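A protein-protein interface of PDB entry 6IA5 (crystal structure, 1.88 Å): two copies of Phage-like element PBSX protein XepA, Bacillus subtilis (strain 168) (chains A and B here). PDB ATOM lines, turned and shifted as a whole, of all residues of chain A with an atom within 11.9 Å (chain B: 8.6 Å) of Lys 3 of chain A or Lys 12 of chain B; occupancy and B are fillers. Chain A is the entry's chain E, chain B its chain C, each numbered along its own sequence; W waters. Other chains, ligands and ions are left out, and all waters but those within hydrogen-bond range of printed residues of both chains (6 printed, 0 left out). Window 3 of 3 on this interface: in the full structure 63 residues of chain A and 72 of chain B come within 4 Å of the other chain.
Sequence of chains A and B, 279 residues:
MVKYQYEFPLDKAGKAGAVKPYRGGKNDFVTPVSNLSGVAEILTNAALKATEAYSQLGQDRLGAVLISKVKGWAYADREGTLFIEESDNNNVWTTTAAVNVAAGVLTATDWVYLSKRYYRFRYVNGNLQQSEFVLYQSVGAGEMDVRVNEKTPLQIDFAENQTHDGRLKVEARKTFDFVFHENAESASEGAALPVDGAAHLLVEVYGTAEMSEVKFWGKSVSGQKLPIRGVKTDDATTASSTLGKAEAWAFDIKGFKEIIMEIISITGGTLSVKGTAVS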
ATOM      1  N   MET A   1       1.451  20.545   5.869  1.00  0.00           N
ATOM      2  CA  MET A   1       0.586  19.356   6.126  1.00  0.00           C
ATOM      3  C   MET A   1       0.904  18.280   5.087  1.00  0.00           C
ATOM      4  O   MET A   1       0.149  18.125   4.125  1.00  0.00           O
ATOM      5  CB  MET A   1      -0.894  19.748   6.016  1.00  0.00           C
ATOM      6  N   VAL A   2       2.021  17.545   5.277  1.00  0.00           N
ATOM      7  CA  VAL A   2       2.413  16.489   4.351  1.00  0.00           C
ATOM      8  C   VAL A   2       1.827  15.126   4.738  1.00  0.00           C
ATOM      9  O   VAL A   2       1.579  14.807   5.907  1.00  0.00           O
ATOM     10  CB  VAL A   2       3.926  16.415   4.046  1.00  0.00           C
ATOM     11  CG1 VAL A   2       4.668  15.370   4.887  1.00  0.00           C
ATOM     12  CG2 VAL A   2       4.135  16.113   2.567  1.00  0.00           C
ATOM     13  N   LYS A   3       1.649  14.309   3.697  1.00  0.00           N
ATOM     14  CA  LYS A   3       1.119  12.955   3.774  1.00  0.00           C
ATOM     15  C   LYS A   3       2.282  11.967   3.801  1.00  0.00           C
ATOM     16  O   LYS A   3       3.273  12.171   3.112  1.00  0.00           O
ATOM     17  CB  LYS A   3       0.158  12.721   2.605  1.00  0.00           C
ATOM     18  CG  LYS A   3      -1.103  13.567   2.643  1.00  0.00           C
ATOM     19  CD  LYS A   3      -2.022  13.358   1.496  1.00  0.00           C
ATOM     20  CE  LYS A   3      -2.975  14.528   1.428  1.00  0.00           C
ATOM     21  NZ  LYS A   3      -4.219  14.191   0.693  1.00  0.00           N
ATOM     22  N   TYR A   4       2.165  10.925   4.639  1.00  0.00           N
ATOM     23  CA  TYR A   4       3.226   9.938   4.827  1.00  0.00           C
ATOM     24  C   TYR A   4       2.910   8.688   4.011  1.00  0.00           C
ATOM     25  O   TYR A   4       1.854   8.618   3.386  1.00  0.00           O
ATOM     26  CB  TYR A   4       3.400   9.613   6.313  1.00  0.00           C
ATOM     27  CG  TYR A   4       4.122  10.697   7.076  1.00  0.00           C
ATOM     28  CD1 TYR A   4       3.506  11.907   7.369  1.00  0.00           C
ATOM     29  CD2 TYR A   4       5.446  10.522   7.470  1.00  0.00           C
ATOM     30  CE1 TYR A   4       4.187  12.929   8.004  1.00  0.00           C
ATOM     31  CE2 TYR A   4       6.134  11.522   8.143  1.00  0.00           C
ATOM     32  CZ  TYR A   4       5.499  12.731   8.405  1.00  0.00           C
ATOM     33  OH  TYR A   4       6.145  13.745   9.053  1.00  0.00           O
ATOM     34  N   GLN A   5       3.808   7.694   4.078  1.00  0.00           N
ATOM     35  CA  GLN A   5       3.733   6.517   3.233  1.00  0.00           C
ATOM     36  C   GLN A   5       2.874   5.417   3.856  1.00  0.00           C
ATOM     37  O   GLN A   5       2.457   4.495   3.164  1.00  0.00           O
ATOM     38  CB  GLN A   5       5.123   5.995   2.894  1.00  0.00           C
ATOM     39  CG  GLN A   5       5.884   6.946   1.984  1.00  0.00           C
ATOM     40  CD  GLN A   5       7.082   7.533   2.680  1.00  0.00           C
ATOM     41  OE1 GLN A   5       8.223   7.155   2.427  1.00  0.00           O
ATOM     42  NE2 GLN A   5       6.820   8.445   3.598  1.00  0.00           N
ATOM     43  N   TYR A   6       2.595   5.496   5.152  1.00  0.00           N
ATOM     44  CA  TYR A   6       1.734   4.473   5.760  1.00  0.00           C
ATOM     45  C   TYR A   6       0.275   4.875   5.547  1.00  0.00           C
ATOM     46  O   TYR A   6      -0.019   6.048   5.345  1.00  0.00           O
ATOM     47  CB  TYR A   6       2.011   4.291   7.261  1.00  0.00           C
ATOM     48  CG  TYR A   6       1.828   5.561   8.045  1.00  0.00           C
ATOM     49  CD1 TYR A   6       0.572   5.962   8.487  1.00  0.00           C
ATOM     50  CD2 TYR A   6       2.899   6.424   8.261  1.00  0.00           C
ATOM     51  CE1 TYR A   6       0.402   7.162   9.163  1.00  0.00           C
ATOM     52  CE2 TYR A   6       2.741   7.624   8.947  1.00  0.00           C
ATOM     53  CZ  TYR A   6       1.489   7.980   9.412  1.00  0.00           C
ATOM     54  OH  TYR A   6       1.336   9.192  10.032  1.00  0.00           O
ATOM     55  N   GLU A   7      -0.638   3.906   5.627  1.00  0.00           N
ATOM     56  CA  GLU A   7      -2.048   4.204   5.461  1.00  0.00           C
ATOM     57  C   GLU A   7      -2.874   3.502   6.536  1.00  0.00           C
ATOM     58  O   GLU A   7      -2.744   2.301   6.724  1.00  0.00           O
ATOM     59  CB  GLU A   7      -2.497   3.739   4.067  1.00  0.00           C
ATOM     60  CG  GLU A   7      -3.858   4.291   3.652  1.00  0.00           C
ATOM     61  CD  GLU A   7      -4.092   4.338   2.144  1.00  0.00           C
ATOM     62  OE1 GLU A   7      -3.126   4.073   1.381  1.00  0.00           O
ATOM     63  OE2 GLU A   7      -5.229   4.641   1.745  1.00  0.00           O
ATOM     64  N   PHE A   8      -3.740   4.258   7.216  1.00  0.00           N
ATOM     65  CA  PHE A   8      -4.573   3.650   8.236  1.00  0.00           C
ATOM     66  C   PHE A   8      -5.574   2.697   7.588  1.00  0.00           C
ATOM     67  O   PHE A   8      -6.210   3.055   6.607  1.00  0.00           O
ATOM     68  CB  PHE A   8      -5.278   4.721   9.061  1.00  0.00           C
ATOM     69  CG  PHE A   8      -4.339   5.583   9.870  1.00  0.00           C
ATOM     70  CD1 PHE A   8      -3.232   5.040  10.530  1.00  0.00           C
ATOM     71  CD2 PHE A   8      -4.606   6.931  10.023  1.00  0.00           C
ATOM     72  CE1 PHE A   8      -2.400   5.847  11.290  1.00  0.00           C
ATOM     73  CE2 PHE A   8      -3.763   7.742  10.777  1.00  0.00           C
ATOM     74  CZ  PHE A   8      -2.651   7.200  11.398  1.00  0.00           C
ATOM     75  N   PRO A   9      -5.753   1.464   8.110  1.00  0.00           N
ATOM     76  CA  PRO A   9      -6.809   0.577   7.603  1.00  0.00           C
ATOM     77  C   PRO A   9      -8.175   1.146   7.986  1.00  0.00           C
ATOM     78  O   PRO A   9      -8.271   2.013   8.865  1.00  0.00           O
ATOM     79  CB  PRO A   9      -6.561  -0.752   8.348  1.00  0.00           C
ATOM     80  CG  PRO A   9      -5.865  -0.292   9.635  1.00  0.00           C
ATOM     81  CD  PRO A   9      -4.976   0.871   9.223  1.00  0.00           C
ATOM     82  N   LEU A  10      -9.225   0.660   7.317  1.00  0.00           N
ATOM     83  CA  LEU A  10     -10.595   1.083   7.584  1.00  0.00           C
ATOM     84  C   LEU A  10     -11.313  -0.103   8.213  1.00  0.00           C
ATOM     85  O   LEU A  10     -11.034  -1.235   7.839  1.00  0.00           O
ATOM     86  CB  LEU A  10     -11.278   1.448   6.250  1.00  0.00           C
ATOM     87  CG  LEU A  10     -10.613   2.512   5.375  1.00  0.00           C
ATOM     88  CD1 LEU A  10     -11.439   2.757   4.116  1.00  0.00           C
ATOM     89  CD2 LEU A  10     -10.432   3.820   6.119  1.00  0.00           C
ATOM     90  N   ALA A  16     -11.484   4.891   9.533  1.00  0.00           N
ATOM     91  CA  ALA A  16     -10.035   4.783   9.643  1.00  0.00           C
ATOM     92  C   ALA A  16      -9.655   4.754  11.124  1.00  0.00           C
ATOM     93  O   ALA A  16     -10.314   5.381  11.948  1.00  0.00           O
ATOM     94  CB  ALA A  16      -9.359   5.946   8.953  1.00  0.00           C
ATOM     95  N   GLY A  17      -8.590   4.018  11.455  1.00  0.00           N
ATOM     96  CA  GLY A  17      -8.070   3.973  12.817  1.00  0.00           C
ATOM     97  C   GLY A  17      -6.595   3.565  12.774  1.00  0.00           C
ATOM     98  O   GLY A  17      -6.174   2.870  11.838  1.00  0.00           O
ATOM     99  N   ALA A  18      -5.825   4.001  13.791  1.00  0.00           N
ATOM    100  CA  ALA A  18      -4.423   3.627  13.860  1.00  0.00           C
ATOM    101  C   ALA A  18      -4.276   2.249  14.510  1.00  0.00           C
ATOM    102  O   ALA A  18      -3.677   2.128  15.576  1.00  0.00           O
ATOM    103  CB  ALA A  18      -3.637   4.701  14.578  1.00  0.00           C
ATOM    104  N   PHE B   8       0.478  16.752  14.018  1.00  0.00           N
ATOM    105  CA  PHE B   8       0.223  15.351  13.734  1.00  0.00           C
ATOM    106  C   PHE B   8       0.559  15.060  12.277  1.00  0.00           C
ATOM    107  O   PHE B   8       0.155  15.805  11.398  1.00  0.00           O
ATOM    108  CB  PHE B   8      -1.229  14.985  14.053  1.00  0.00           C
ATOM    109  CG  PHE B   8      -1.582  15.115  15.515  1.00  0.00           C
ATOM    110  CD1 PHE B   8      -0.705  14.657  16.499  1.00  0.00           C
ATOM    111  CD2 PHE B   8      -2.785  15.696  15.915  1.00  0.00           C
ATOM    112  CE1 PHE B   8      -1.021  14.779  17.843  1.00  0.00           C
ATOM    113  CE2 PHE B   8      -3.100  15.818  17.261  1.00  0.00           C
ATOM    114  CZ  PHE B   8      -2.232  15.334  18.221  1.00  0.00           C
ATOM    115  N   PRO B   9       1.285  13.964  11.962  1.00  0.00           N
ATOM    116  CA  PRO B   9       1.460  13.542  10.569  1.00  0.00           C
ATOM    117  C   PRO B   9       0.120  13.102   9.981  1.00  0.00           C
ATOM    118  O   PRO B   9      -0.821  12.800  10.716  1.00  0.00           O
ATOM    119  CB  PRO B   9       2.418  12.343  10.659  1.00  0.00           C
ATOM    120  CG  PRO B   9       2.210  11.818  12.057  1.00  0.00           C
ATOM    121  CD  PRO B   9       1.938  13.046  12.914  1.00  0.00           C
ATOM    122  N   LEU B  10       0.049  13.076   8.642  1.00  0.00           N
ATOM    123  CA  LEU B  10      -1.122  12.600   7.923  1.00  0.00           C
ATOM    124  C   LEU B  10      -0.713  11.292   7.261  1.00  0.00           C
ATOM    125  O   LEU B  10       0.436  11.155   6.843  1.00  0.00           O
ATOM    126  CB  LEU B  10      -1.509  13.631   6.852  1.00  0.00           C
ATOM    127  CG  LEU B  10      -1.789  15.067   7.310  1.00  0.00           C
ATOM    128  CD1 LEU B  10      -2.184  15.925   6.104  1.00  0.00           C
ATOM    129  CD2 LEU B  10      -2.904  15.123   8.341  1.00  0.00           C
ATOM    130  N   ASP B  11      -1.645  10.336   7.161  1.00  0.00           N
ATOM    131  CA  ASP B  11      -1.367   9.124   6.409  1.00  0.00           C
ATOM    132  C   ASP B  11      -1.502   9.409   4.906  1.00  0.00           C
ATOM    133  O   ASP B  11      -1.724  10.553   4.492  1.00  0.00           O
ATOM    134  CB  ASP B  11      -2.228   7.945   6.881  1.00  0.00           C
ATOM    135  CG  ASP B  11      -3.642   7.917   6.305  1.00  0.00           C
ATOM    136  OD1 ASP B  11      -4.098   8.966   5.804  1.00  0.00           O
ATOM    137  OD2 ASP B  11      -4.283   6.849   6.370  1.00  0.00           O
ATOM    138  N   LYS B  12      -1.385   8.341   4.100  1.00  0.00           N
ATOM    139  CA  LYS B  12      -1.385   8.437   2.648  1.00  0.00           C
ATOM    140  C   LYS B  12      -2.690   9.072   2.163  1.00  0.00           C
ATOM    141  O   LYS B  12      -2.691   9.810   1.185  1.00  0.00           O
ATOM    142  CB  LYS B  12      -1.163   7.060   2.030  1.00  0.00           C
ATOM    143  CG  LYS B  12      -0.426   7.094   0.710  1.00  0.00           C
ATOM    144  CD  LYS B  12      -0.038   5.731   0.176  1.00  0.00           C
ATOM    145  CE  LYS B  12       1.220   5.806  -0.674  1.00  0.00           C
ATOM    146  NZ  LYS B  12       1.184   4.901  -1.854  1.00  0.00           N
ATOM    147  N   ALA B  13      -3.788   8.814   2.880  1.00  0.00           N
ATOM    148  CA  ALA B  13      -5.114   9.302   2.525  1.00  0.00           C
ATOM    149  C   ALA B  13      -5.389  10.664   3.162  1.00  0.00           C
ATOM    150  O   ALA B  13      -6.528  11.115   3.150  1.00  0.00           O
ATOM    151  CB  ALA B  13      -6.160   8.278   2.936  1.00  0.00           C
ATOM    152  N   GLY B  14      -4.370  11.288   3.764  1.00  0.00           N
ATOM    153  CA  GLY B  14      -4.542  12.582   4.411  1.00  0.00           C
ATOM    154  C   GLY B  14      -5.199  12.535   5.797  1.00  0.00           C
ATOM    155  O   GLY B  14      -5.600  13.577   6.305  1.00  0.00           O
ATOM    156  N   LYS B  15      -5.279  11.360   6.443  1.00  0.00           N
ATOM    157  CA  LYS B  15      -5.860  11.274   7.783  1.00  0.00           C
ATOM    158  C   LYS B  15      -4.803  11.506   8.865  1.00  0.00           C
ATOM    159  O   LYS B  15      -3.746  10.866   8.857  1.00  0.00           O
ATOM    160  CB  LYS B  15      -6.579   9.938   7.973  1.00  0.00           C
ATOM    161  CG  LYS B  15      -7.760   9.736   7.037  1.00  0.00           C
ATOM    162  CD  LYS B  15      -8.041   8.286   6.715  1.00  0.00           C
ATOM    163  CE  LYS B  15      -9.173   8.111   5.724  1.00  0.00           C
ATOM    164  NZ  LYS B  15     -10.371   8.899   6.109  1.00  0.00           N
ATOM    165  N   ALA B  16      -5.092  12.461   9.769  1.00  0.00           N
ATOM    166  CA  ALA B  16      -4.202  12.797  10.875  1.00  0.00           C
ATOM    167  C   ALA B  16      -4.243  11.686  11.932  1.00  0.00           C
ATOM    168  O   ALA B  16      -5.259  11.034  12.115  1.00  0.00           O
ATOM    169  CB  ALA B  16      -4.614  14.116  11.482  1.00  0.00           C
ATOM    170  N   GLY B  25      10.735   1.442   4.860  1.00  0.00           N
ATOM    171  CA  GLY B  25       9.931   2.245   3.956  1.00  0.00           C
ATOM    172  C   GLY B  25       8.903   3.154   4.641  1.00  0.00           C
ATOM    173  O   GLY B  25       8.047   3.721   3.960  1.00  0.00           O
ATOM    174  N   LYS B  26       8.978   3.292   5.976  1.00  0.00           N
ATOM    175  CA  LYS B  26       8.132   4.214   6.731  1.00  0.00           C
ATOM    176  C   LYS B  26       6.661   3.982   6.412  1.00  0.00           C
ATOM    177  O   LYS B  26       5.861   4.917   6.370  1.00  0.00           O
ATOM    178  CB  LYS B  26       8.554   5.675   6.479  1.00  0.00           C
ATOM    179  CG  LYS B  26       9.992   5.962   6.870  1.00  0.00           C
ATOM    180  CD  LYS B  26      10.218   5.577   8.324  1.00  0.00           C
ATOM    181  CE  LYS B  26      11.647   5.731   8.792  1.00  0.00           C
ATOM    182  NZ  LYS B  26      12.388   4.453   8.651  1.00  0.00           N
ATOM    183  N   ASN B  27       6.307   2.715   6.221  1.00  0.00           N
ATOM    184  CA  ASN B  27       4.962   2.375   5.798  1.00  0.00           C
ATOM    185  C   ASN B  27       4.204   1.693   6.932  1.00  0.00           C
ATOM    186  O   ASN B  27       3.160   1.096   6.694  1.00  0.00           O
ATOM    187  CB  ASN B  27       4.999   1.486   4.551  1.00  0.00           C
ATOM    188  CG  ASN B  27       5.771   0.207   4.791  1.00  0.00           C
ATOM    189  OD1 ASN B  27       6.649   0.121   5.659  1.00  0.00           O
ATOM    190  ND2 ASN B  27       5.420  -0.817   4.046  1.00  0.00           N
HETATM  191  O   HOH W   1       0.594   1.181   5.744  1.00  0.00           O
HETATM  192  O   HOH W   2     -12.472   7.543   7.958  1.00  0.00           O
HETATM  193  O   HOH W   3      -6.507   5.710   5.921  1.00  0.00           O
HETATM  194  O   HOH W   4       5.903   7.876   6.000  1.00  0.00           O
HETATM  195  O   HOH W   5      -4.275  11.590  -0.132  1.00  0.00           O
HETATM  196  O   HOH W   6      -1.103   9.967  10.435  1.00  0.00           O
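Of the printed residues of chain A, Lys 12 of chain B touches Lys 3 (3.6 Å), Tyr 4 (3.3 Å), Tyr 6 (2.9 Å) and Glu 7 (3.6 Å).
Val 2 of chain A touches just one residue of chain B: Leu 10.
Printed residues of chain A within 4 Å of Asp 11 of chain B: Lys 3 (3.4 Å), Tyr 4 (3.8 Å), Tyr 6 (3.3 Å), Glu 7 (3.6 Å) and Phe 8 (2.8 Å).
Of chain A, only Glu 7 comes within 4 Å of Ala 13 of chain B.
Of the printed residues of chain B, Phe 8 of chain A touches Asp 11, Lys 15 and Ala 16.
Of the printed residues of chain B, Glu 7 of chain A touches Asp 11 (3.6 Å), Lys 12 (3.6 Å) and Ala 13 (3.9 Å).
Printed residues of chain A within 4 Å of Asn 27 of chain B: Tyr 6.
Of the printed residues of chain A, Lys 26 of chain B touches Gln 5 and Tyr 6.
Printed residues of chain A within 4 Å of Lys 15 of chain B: Phe 8 and Ala 16.
Phe 8 of chain B touches none of the printed residues of chain A.
The nearest residue of chain B that does not touch Lys 3 of chain A is Ala 13 of chain B (4.5 Å).
Hydrophobic or aromatic side chains of chain B within 4 Å of the printed part of chain A: Pro 9, Leu 10 and Ala 13.
Printed residues of chain A that touch a printed residue of chain B: Met 1, Val 2, Lys 3, Tyr 4, Gln 5, Tyr 6, Glu 7, Phe 8 and Ala 16.
Among the printed residues, no Asp or Glu carboxylate lies within 4 Å of a Lys or Arg side-chain nitrogen of the other chain.
O of Leu 10 of chain B lies within hydrogen-bond range of N of Tyr 4 of chain A, 2.8 Å away.
N of Lys 12 of chain B sits close to O of Tyr 4 of chain A (3.3 Å).
The side-chain carboxylate of Asp 11 of chain B sits at hydrogen-bond distance from the backbone NH of Phe 8 of chain A, 2.8 Å away.
O of Tyr 6 of chain A sits at hydrogen-bond distance from N of Lys 12 of chain B (2.9 Å).
Water W3 bridges OD2 of Asp 11 of chain B and O of Phe 8 of chain A.
Water W6 lies within hydrogen-bond range of the side-chain hydroxyl (OH) of Tyr 6 of chain A (2.6 Å), the backbone carbonyl oxygen (O) of Pro 9 of chain B (2.9 Å), the backbone carbonyl oxygen (O) of Lys 15 of chain B (3.2 Å) and the backbone NH (N) of Asp 11 of chain B (3.3 Å).
Water W4 bridges the side-chain amide nitrogen of Gln 5 of chain A and the backbone carbonyl oxygen of Lys 26 of chain B.
Water W5 lies within hydrogen-bond range of the backbone carbonyl oxygen (O) of Lys 12 of chain B (2.7 Å) and the side-chain amino group (NZ) of Lys 3 of chain A (2.7 Å).
Water W1 lies within hydrogen-bond range of O of Asn 27 of chain B (2.7 Å) and N of Glu 7 of chain A (3.0 Å).
Water W2 lies within hydrogen-bond range of the side-chain amino group of Lys 15 of chain B (3.1 Å) and the backbone NH of Ala 16 of chain A (3.2 Å).
Among the printed residues, merely in contact across the chains: Tyr 4 of chain A with Pro 9 of chain B (3.2 Å), Tyr 6 of chain A with Asp 11 of chain B (3.3 Å), Tyr 6 of chain A with Pro 9 of chain B (3.4 Å), Tyr 6 of chain A with Asn 27 of chain B (3.4 Å), Lys 3 of chain A with Asp 11 of chain B (3.4 Å), Val 2 of chain A with Leu 10 of chain B (3.4 Å), Ala 16 of chain A with Lys 15 of chain B (3.5 Å), Tyr 6 of chain A with Lys 26 of chain B (3.5 Å), Glu 7 of chain A with Asp 11 of chain B (3.6 Å), Lys 3 of chain A with Leu 10 of chain B (3.6 Å), Lys 3 of chain A with Lys 12 of chain B (3.6 Å), Glu 7 of chain A with Lys 12 of chain B (3.6 Å), Phe 8 of chain A with Lys 15 of chain B (3.7 Å), Gln 5 of chain A with Lys 26 of chain B (3.7 Å), Gln 5 of chain A with Gly 25 of chain B (3.8 Å), Tyr 4 of chain A with Asp 11 of chain B (3.8 Å), Met 1 of chain A with Leu 10 of chain B (3.8 Å), Tyr 6 of chain A with Leu 10 of chain B (3.9 Å), Phe 8 of chain A with Ala 16 of chain B (3.9 Å), Lys 3 of chain A with Gly 14 of chain B (3.9 Å) and Glu 7 of chain A with Ala 13 of chain B (3.9 Å).
The side-chain carboxylate (OD1) of Asp 11 of chain B is in hydrogen-bond range of the backbone NH (N) of Lys 15 of chain B (2.7 Å).
The side-chain carboxylate (OD1) of Asp 11 of chain B is in hydrogen-bond range of the backbone NH (N) of Gly 14 of chain B, at 3.1 Å.
OD1 of Asp 11 of chain B sits at hydrogen-bond distance from N of Ala 13 of chain B.
Phe 8 of chain A touches Ala 16 of chain B, but with the chains exchanged Ala 16 of chain A does not touch Phe 8 of chain B (13.2 Å).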
